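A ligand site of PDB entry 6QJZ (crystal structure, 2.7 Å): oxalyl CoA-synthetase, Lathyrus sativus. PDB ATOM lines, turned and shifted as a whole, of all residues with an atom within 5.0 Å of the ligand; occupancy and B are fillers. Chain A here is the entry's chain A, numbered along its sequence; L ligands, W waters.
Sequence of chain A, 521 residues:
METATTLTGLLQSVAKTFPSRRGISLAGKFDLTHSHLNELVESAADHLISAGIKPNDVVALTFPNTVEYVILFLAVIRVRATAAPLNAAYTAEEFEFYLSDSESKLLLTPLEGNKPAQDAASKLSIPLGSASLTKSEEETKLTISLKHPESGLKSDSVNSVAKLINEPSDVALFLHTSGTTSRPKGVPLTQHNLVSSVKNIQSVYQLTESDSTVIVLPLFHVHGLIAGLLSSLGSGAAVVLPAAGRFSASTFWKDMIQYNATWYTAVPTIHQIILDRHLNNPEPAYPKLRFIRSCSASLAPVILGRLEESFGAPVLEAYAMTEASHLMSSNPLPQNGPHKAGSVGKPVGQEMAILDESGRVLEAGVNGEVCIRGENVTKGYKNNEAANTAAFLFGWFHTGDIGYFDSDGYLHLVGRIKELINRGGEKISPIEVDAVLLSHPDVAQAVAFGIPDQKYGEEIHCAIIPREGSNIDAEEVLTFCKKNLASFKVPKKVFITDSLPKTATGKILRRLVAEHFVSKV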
ATOM      1  N   THR A 177     -35.667   9.674  18.707  1.00  0.00           N
ATOM      2  CA  THR A 177     -34.360  10.323  18.990  1.00  0.00           C
ATOM      3  C   THR A 177     -34.192  11.490  18.013  1.00  0.00           C
ATOM      4  O   THR A 177     -34.929  11.524  17.009  1.00  0.00           O
ATOM      5  CB  THR A 177     -33.230   9.285  18.917  1.00  0.00           C
ATOM      6  OG1 THR A 177     -32.072   9.866  19.520  1.00  0.00           O
ATOM      7  CG2 THR A 177     -32.908   8.858  17.498  1.00  0.00           C
ATOM      8  N   HIS A 221     -36.891   5.458  29.118  1.00  0.00           N
ATOM      9  CA  HIS A 221     -35.539   5.616  28.493  1.00  0.00           C
ATOM     10  C   HIS A 221     -34.790   4.277  28.605  1.00  0.00           C
ATOM     11  O   HIS A 221     -35.026   3.546  29.575  1.00  0.00           O
ATOM     12  CB  HIS A 221     -34.790   6.793  29.138  1.00  0.00           C
ATOM     13  CG  HIS A 221     -33.487   7.116  28.467  1.00  0.00           C
ATOM     14  ND1 HIS A 221     -32.282   6.579  28.896  1.00  0.00           N
ATOM     15  CD2 HIS A 221     -33.203   7.904  27.416  1.00  0.00           C
ATOM     16  CE1 HIS A 221     -31.311   7.029  28.124  1.00  0.00           C
ATOM     17  NE2 HIS A 221     -31.857   7.850  27.203  1.00  0.00           N
ATOM     18  N   VAL A 222     -33.922   3.992  27.630  1.00  0.00           N
ATOM     19  CA  VAL A 222     -33.245   2.676  27.459  1.00  0.00           C
ATOM     20  C   VAL A 222     -32.375   2.361  28.695  1.00  0.00           C
ATOM     21  O   VAL A 222     -32.305   1.177  29.059  1.00  0.00           O
ATOM     22  CB  VAL A 222     -32.430   2.605  26.149  1.00  0.00           C
ATOM     23  CG1 VAL A 222     -33.348   2.568  24.941  1.00  0.00           C
ATOM     24  CG2 VAL A 222     -31.416   3.737  26.029  1.00  0.00           C
ATOM     25  N   CYS A 295     -23.952   6.493  33.661  1.00  0.00           N
ATOM     26  CA  CYS A 295     -24.184   6.471  32.186  1.00  0.00           C
ATOM     27  C   CYS A 295     -24.914   7.757  31.755  1.00  0.00           C
ATOM     28  O   CYS A 295     -25.249   8.556  32.646  1.00  0.00           O
ATOM     29  CB  CYS A 295     -24.993   5.239  31.802  1.00  0.00           C
ATOM     30  SG  CYS A 295     -24.563   4.535  30.196  1.00  0.00           S
ATOM     31  N   SER A 296     -25.091   7.944  30.448  1.00  0.00           N
ATOM     32  CA  SER A 296     -26.017   8.919  29.805  1.00  0.00           C
ATOM     33  C   SER A 296     -25.407  10.328  29.731  1.00  0.00           C
ATOM     34  O   SER A 296     -25.747  11.065  28.770  1.00  0.00           O
ATOM     35  CB  SER A 296     -27.351   8.942  30.508  1.00  0.00           C
ATOM     36  OG  SER A 296     -27.844   7.626  30.714  1.00  0.00           O
ATOM     37  N   ALA A 297     -24.581  10.706  30.704  1.00  0.00           N
ATOM     38  CA  ALA A 297     -23.868  12.007  30.769  1.00  0.00           C
ATOM     39  C   ALA A 297     -22.513  11.802  31.448  1.00  0.00           C
ATOM     40  O   ALA A 297     -22.441  10.948  32.353  1.00  0.00           O
ATOM     41  CB  ALA A 297     -24.709  13.025  31.508  1.00  0.00           C
ATOM     42  N   SER A 298     -21.491  12.553  31.035  1.00  0.00           N
ATOM     43  CA  SER A 298     -20.104  12.387  31.534  1.00  0.00           C
ATOM     44  C   SER A 298     -20.080  12.596  33.050  1.00  0.00           C
ATOM     45  O   SER A 298     -20.626  13.616  33.517  1.00  0.00           O
ATOM     46  CB  SER A 298     -19.140  13.303  30.826  1.00  0.00           C
ATOM     47  OG  SER A 298     -19.426  14.661  31.112  1.00  0.00           O
ATOM     48  N   GLU A 317     -18.290   3.759  34.927  1.00  0.00           N
ATOM     49  CA  GLU A 317     -18.926   4.661  33.920  1.00  0.00           C
ATOM     50  C   GLU A 317     -19.067   3.901  32.591  1.00  0.00           C
ATOM     51  O   GLU A 317     -18.090   3.272  32.158  1.00  0.00           O
ATOM     52  CB  GLU A 317     -18.115   5.940  33.723  1.00  0.00           C
ATOM     53  CG  GLU A 317     -18.841   6.967  32.852  1.00  0.00           C
ATOM     54  CD  GLU A 317     -18.258   8.368  32.827  1.00  0.00           C
ATOM     55  OE1 GLU A 317     -17.142   8.563  33.370  1.00  0.00           O
ATOM     56  OE2 GLU A 317     -18.927   9.262  32.261  1.00  0.00           O
ATOM     57  N   ALA A 318     -20.252   3.983  31.976  1.00  0.00           N
ATOM     58  CA  ALA A 318     -20.583   3.302  30.705  1.00  0.00           C
ATOM     59  C   ALA A 318     -21.091   4.337  29.682  1.00  0.00           C
ATOM     60  O   ALA A 318     -21.328   5.499  30.065  1.00  0.00           O
ATOM     61  CB  ALA A 318     -21.609   2.219  30.951  1.00  0.00           C
ATOM     62  N   TYR A 319     -21.231   3.892  28.432  1.00  0.00           N
ATOM     63  CA  TYR A 319     -21.618   4.713  27.253  1.00  0.00           C
ATOM     64  C   TYR A 319     -22.680   3.945  26.469  1.00  0.00           C
ATOM     65  O   TYR A 319     -22.401   2.819  26.004  1.00  0.00           O
ATOM     66  CB  TYR A 319     -20.351   5.040  26.443  1.00  0.00           C
ATOM     67  CG  TYR A 319     -20.541   5.559  25.040  1.00  0.00           C
ATOM     68  CD1 TYR A 319     -21.246   6.724  24.780  1.00  0.00           C
ATOM     69  CD2 TYR A 319     -19.938   4.921  23.962  1.00  0.00           C
ATOM     70  CE1 TYR A 319     -21.377   7.217  23.498  1.00  0.00           C
ATOM     71  CE2 TYR A 319     -20.062   5.398  22.679  1.00  0.00           C
ATOM     72  CZ  TYR A 319     -20.785   6.548  22.436  1.00  0.00           C
ATOM     73  OH  TYR A 319     -20.899   7.017  21.158  1.00  0.00           O
ATOM     74  N   ALA A 320     -23.882   4.515  26.377  1.00  0.00           N
ATOM     75  CA  ALA A 320     -25.083   3.866  25.810  1.00  0.00           C
ATOM     76  C   ALA A 320     -25.868   4.877  24.963  1.00  0.00           C
ATOM     77  O   ALA A 320     -25.727   6.093  25.195  1.00  0.00           O
ATOM     78  CB  ALA A 320     -25.924   3.304  26.926  1.00  0.00           C
ATOM     79  N   MET A 321     -26.666   4.364  24.024  1.00  0.00           N
ATOM     80  CA  MET A 321     -27.641   5.177  23.235  1.00  0.00           C
ATOM     81  C   MET A 321     -28.769   4.273  22.742  1.00  0.00           C
ATOM     82  O   MET A 321     -28.588   3.037  22.706  1.00  0.00           O
ATOM     83  CB  MET A 321     -26.954   5.877  22.062  1.00  0.00           C
ATOM     84  CG  MET A 321     -26.477   4.933  20.974  1.00  0.00           C
ATOM     85  SD  MET A 321     -25.355   5.775  19.830  1.00  0.00           S
ATOM     86  CE  MET A 321     -26.400   7.115  19.264  1.00  0.00           C
ATOM     87  N   THR A 322     -29.896   4.892  22.370  1.00  0.00           N
ATOM     88  CA  THR A 322     -31.175   4.219  22.026  1.00  0.00           C
ATOM     89  C   THR A 322     -30.975   3.316  20.799  1.00  0.00           C
ATOM     90  O   THR A 322     -31.395   2.143  20.855  1.00  0.00           O
ATOM     91  CB  THR A 322     -32.281   5.263  21.822  1.00  0.00           C
ATOM     92  OG1 THR A 322     -32.214   6.165  22.919  1.00  0.00           O
ATOM     93  CG2 THR A 322     -33.666   4.648  21.731  1.00  0.00           C
ATOM     94  N   GLU A 323     -30.311   3.828  19.757  1.00  0.00           N
ATOM     95  CA  GLU A 323     -30.073   3.106  18.478  1.00  0.00           C
ATOM     96  C   GLU A 323     -29.252   1.837  18.726  1.00  0.00           C
ATOM     97  O   GLU A 323     -29.384   0.890  17.936  1.00  0.00           O
ATOM     98  CB  GLU A 323     -29.376   4.013  17.467  1.00  0.00           C
ATOM     99  CG  GLU A 323     -30.235   5.184  17.004  1.00  0.00           C
ATOM    100  CD  GLU A 323     -30.063   6.474  17.786  1.00  0.00           C
ATOM    101  OE1 GLU A 323     -29.888   6.396  19.024  1.00  0.00           O
ATOM    102  OE2 GLU A 323     -30.100   7.557  17.167  1.00  0.00           O
ATOM    103  N   VAL A 344     -15.230   5.756  29.310  1.00  0.00           N
ATOM    104  CA  VAL A 344     -16.485   4.940  29.271  1.00  0.00           C
ATOM    105  C   VAL A 344     -16.144   3.480  28.951  1.00  0.00           C
ATOM    106  O   VAL A 344     -17.049   2.715  28.589  1.00  0.00           O
ATOM    107  CB  VAL A 344     -17.495   5.547  28.276  1.00  0.00           C
ATOM    108  CG1 VAL A 344     -17.999   6.904  28.743  1.00  0.00           C
ATOM    109  CG2 VAL A 344     -16.941   5.653  26.860  1.00  0.00           C
ATOM    110  N   THR A 399     -22.577   7.380  15.703  1.00  0.00           N
ATOM    111  CA  THR A 399     -23.198   7.739  17.008  1.00  0.00           C
ATOM    112  C   THR A 399     -23.518   9.241  17.054  1.00  0.00           C
ATOM    113  O   THR A 399     -24.489   9.616  17.740  1.00  0.00           O
ATOM    114  CB  THR A 399     -22.296   7.389  18.201  1.00  0.00           C
ATOM    115  OG1 THR A 399     -21.103   8.178  18.107  1.00  0.00           O
ATOM    116  CG2 THR A 399     -21.956   5.908  18.266  1.00  0.00           C
ATOM    117  N   ASP A 401     -21.120  11.185  18.224  1.00  0.00           N
ATOM    118  CA  ASP A 401     -20.173  11.523  19.319  1.00  0.00           C
ATOM    119  C   ASP A 401     -18.748  11.542  18.766  1.00  0.00           C
ATOM    120  O   ASP A 401     -18.442  10.696  17.910  1.00  0.00           O
ATOM    121  CB  ASP A 401     -20.280  10.517  20.476  1.00  0.00           C
ATOM    122  CG  ASP A 401     -21.662  10.466  21.110  1.00  0.00           C
ATOM    123  OD1 ASP A 401     -22.137  11.529  21.544  1.00  0.00           O
ATOM    124  OD2 ASP A 401     -22.251   9.371  21.133  1.00  0.00           O
ATOM    125  N   LEU A 413     -14.947  10.135  25.473  1.00  0.00           N
ATOM    126  CA  LEU A 413     -15.877  11.059  24.756  1.00  0.00           C
ATOM    127  C   LEU A 413     -15.394  12.488  24.986  1.00  0.00           C
ATOM    128  O   LEU A 413     -15.330  12.898  26.164  1.00  0.00           O
ATOM    129  CB  LEU A 413     -17.303  10.873  25.275  1.00  0.00           C
ATOM    130  CG  LEU A 413     -17.861   9.455  25.194  1.00  0.00           C
ATOM    131  CD1 LEU A 413     -19.243   9.384  25.838  1.00  0.00           C
ATOM    132  CD2 LEU A 413     -17.922   8.975  23.751  1.00  0.00           C
ATOM    133  N   ARG A 416     -19.123  16.283  20.311  1.00  0.00           N
ATOM    134  CA  ARG A 416     -20.327  15.805  19.579  1.00  0.00           C
ATOM    135  C   ARG A 416     -20.387  16.457  18.198  1.00  0.00           C
ATOM    136  O   ARG A 416     -20.185  17.685  18.100  1.00  0.00           O
ATOM    137  CB  ARG A 416     -21.590  16.123  20.384  1.00  0.00           C
ATOM    138  CG  ARG A 416     -21.767  15.267  21.627  1.00  0.00           C
ATOM    139  CD  ARG A 416     -23.195  15.268  22.132  1.00  0.00           C
ATOM    140  NE  ARG A 416     -23.636  16.592  22.549  1.00  0.00           N
ATOM    141  CZ  ARG A 416     -23.412  17.145  23.736  1.00  0.00           C
ATOM    142  NH1 ARG A 416     -22.739  16.495  24.680  1.00  0.00           N
ATOM    143  NH2 ARG A 416     -23.877  18.358  23.989  1.00  0.00           N
ATOM    144  N   LYS A 418     -23.276  15.706  16.218  1.00  0.00           N
ATOM    145  CA  LYS A 418     -24.734  15.985  16.292  1.00  0.00           C
ATOM    146  C   LYS A 418     -24.974  17.170  17.245  1.00  0.00           C
ATOM    147  O   LYS A 418     -24.139  17.393  18.141  1.00  0.00           O
ATOM    148  CB  LYS A 418     -25.500  14.741  16.757  1.00  0.00           C
ATOM    149  CG  LYS A 418     -25.200  14.270  18.172  1.00  0.00           C
ATOM    150  CD  LYS A 418     -25.783  12.908  18.488  1.00  0.00           C
ATOM    151  CE  LYS A 418     -25.067  12.222  19.636  1.00  0.00           C
ATOM    152  NZ  LYS A 418     -25.790  11.001  20.059  1.00  0.00           N
ATOM    153  N   LEU A 420     -26.887  18.374  20.197  1.00  0.00           N
ATOM    154  CA  LEU A 420     -27.629  17.962  21.427  1.00  0.00           C
ATOM    155  C   LEU A 420     -27.270  18.923  22.558  1.00  0.00           C
ATOM    156  O   LEU A 420     -26.148  19.456  22.556  1.00  0.00           O
ATOM    157  CB  LEU A 420     -27.234  16.531  21.808  1.00  0.00           C
ATOM    158  CG  LEU A 420     -28.094  15.421  21.210  1.00  0.00           C
ATOM    159  CD1 LEU A 420     -27.547  14.059  21.622  1.00  0.00           C
ATOM    160  CD2 LEU A 420     -29.540  15.562  21.645  1.00  0.00           C
ATOM    161  N   ASN A 422     -27.282  17.990  26.448  1.00  0.00           N
ATOM    162  CA  ASN A 422     -27.432  16.908  27.458  1.00  0.00           C
ATOM    163  C   ASN A 422     -27.651  17.560  28.833  1.00  0.00           C
ATOM    164  O   ASN A 422     -26.659  17.930  29.478  1.00  0.00           O
ATOM    165  CB  ASN A 422     -26.225  15.958  27.434  1.00  0.00           C
ATOM    166  CG  ASN A 422     -26.455  14.675  28.200  1.00  0.00           C
ATOM    167  OD1 ASN A 422     -27.336  14.602  29.054  1.00  0.00           O
ATOM    168  ND2 ASN A 422     -25.658  13.658  27.897  1.00  0.00           N
ATOM    169  N   LYS A 427     -32.048  14.549  26.790  1.00  0.00           N
ATOM    170  CA  LYS A 427     -31.589  15.076  25.486  1.00  0.00           C
ATOM    171  C   LYS A 427     -32.578  16.132  24.992  1.00  0.00           C
ATOM    172  O   LYS A 427     -33.788  15.835  24.921  1.00  0.00           O
ATOM    173  CB  LYS A 427     -31.387  13.930  24.495  1.00  0.00           C
ATOM    174  CG  LYS A 427     -30.025  13.254  24.552  1.00  0.00           C
ATOM    175  CD  LYS A 427     -29.783  12.487  25.838  1.00  0.00           C
ATOM    176  CE  LYS A 427     -28.339  12.049  26.001  1.00  0.00           C
ATOM    177  NZ  LYS A 427     -28.214  10.960  27.000  1.00  0.00           N
HETATM  178  P1  LIG L   1     -29.703   8.441  24.421  1.00  0.00           P
HETATM  179  O1  LIG L   1     -29.227   7.497  25.518  1.00  0.00           O
HETATM  180  O2  LIG L   1     -29.979   7.724  23.113  1.00  0.00           O
HETATM  181  O3  LIG L   1     -30.841   9.331  24.865  1.00  0.00           O
HETATM  182  O4  LIG L   1     -28.459   9.420  24.117  1.00  0.00           O
HETATM  183  C1  LIG L   1     -27.171   8.812  23.824  1.00  0.00           C
HETATM  184  C2  LIG L   1     -26.093   9.862  23.907  1.00  0.00           C
HETATM  185  O5  LIG L   1     -25.796  10.156  25.291  1.00  0.00           O
HETATM  186  C3  LIG L   1     -24.728   9.472  23.344  1.00  0.00           C
HETATM  187  O6  LIG L   1     -24.689   9.575  21.930  1.00  0.00           O
HETATM  188  C4  LIG L   1     -23.833  10.521  24.015  1.00  0.00           C
HETATM  189  O7  LIG L   1     -23.894  11.749  23.343  1.00  0.00           O
HETATM  190  C5  LIG L   1     -24.473  10.631  25.406  1.00  0.00           C
HETATM  191  N1  LIG L   1     -23.784   9.858  26.433  1.00  0.00           N
HETATM  192  C6  LIG L   1     -24.047   8.568  26.824  1.00  0.00           C
HETATM  193  N2  LIG L   1     -23.268   8.150  27.791  1.00  0.00           N
HETATM  194  C7  LIG L   1     -22.436   9.229  28.046  1.00  0.00           C
HETATM  195  C8  LIG L   1     -21.386   9.409  28.967  1.00  0.00           C
HETATM  196  N3  LIG L   1     -20.990   8.477  29.824  1.00  0.00           N
HETATM  197  N4  LIG L   1     -20.768  10.614  28.968  1.00  0.00           N
HETATM  198  C9  LIG L   1     -21.174  11.554  28.106  1.00  0.00           C
HETATM  199  N5  LIG L   1     -22.142  11.491  27.204  1.00  0.00           N
HETATM  200  C10 LIG L   1     -22.743  10.294  27.217  1.00  0.00           C
HETATM  201  O   HOH W   1     -17.566  10.562  29.494  1.00  0.00           O
HETATM  202  O   HOH W   2     -33.422   9.864  24.563  1.00  0.00           O
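The side-chain amino group (NZ) of Lys 427 is in salt-bridge range of an oxygen (O3) of the ligand, at 3.8 Å.
N of Ser 296 sits at hydrogen-bond distance from N2 of the ligand (3.2 Å).
An oxygen (O2) of the ligand lies within hydrogen-bond range of the side-chain hydroxyl (OG1) of Thr 322 (2.7 Å).
N of Ser 298 lies within hydrogen-bond range of N4 of the ligand (2.9 Å).
The side-chain carboxylate of Glu 317 sits at hydrogen-bond distance from a nitrogen (N3) of the ligand, 3.3 Å away.
NZ of Lys 418 is in hydrogen-bond range of O6 of the ligand, at 2.6 Å.
OD1 of Asp 401 lies within hydrogen-bond range of O7 of the ligand, at 2.5 Å.
O3 of the ligand is in hydrogen-bond range of NE2 of His 221.
The backbone carbonyl oxygen of Ala 318 lies within hydrogen-bond range of a nitrogen (N3) of the ligand (3.0 Å).
The backbone NH (N) of Thr 322 lies within hydrogen-bond range of an oxygen (O2) of the ligand (2.9 Å).
NH2 of Arg 416 sits at hydrogen-bond distance from O of Leu 420 (2.9 Å).
O of Ser 296 lies within hydrogen-bond range of ND2 of Asn 422, 2.7 Å away.
The side-chain amino group (NZ) of Lys 418 lies within salt-bridge range of the side-chain carboxylate (OD1) of Asp 401, at 3.98 Å.
The side-chain hydroxyl of Tyr 319 sits at hydrogen-bond distance from the side-chain carboxylate of Asp 401 (2.7 Å).
NZ of Lys 418 sits at hydrogen-bond distance from O of Thr 399 (3.0 Å).
The side-chain hydroxyl (OH) of Tyr 319 lies within hydrogen-bond range of the side-chain hydroxyl (OG1) of Thr 399, 3.3 Å away.
The backbone carbonyl oxygen of Ala 318 is in hydrogen-bond range of the side-chain sulfur of Cys 295.
The backbone NH (N) of Asp 401 lies within hydrogen-bond range of the side-chain hydroxyl (OG1) of Thr 399 (3.0 Å).
Merely in contact with the ligand: Ala 297 (3.3 Å), Ala 320 (3.4 Å), Met 321 (3.4 Å), Val 344 (3.5 Å), Leu 413 (3.7 Å), Arg 416 (3.8 Å) and Tyr 319 (3.9 Å).
Hydrophobic or aromatic side chains within 4 Å of the ligand: His 221, Tyr 319, Met 321, Val 344 and Leu 413.
Of the 23 residues printed, 16 come within 4 Å of the ligand.
Water W1 bridges N4 of the ligand (3.2 Å) and OE2 of Glu 317 (3.3 Å).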
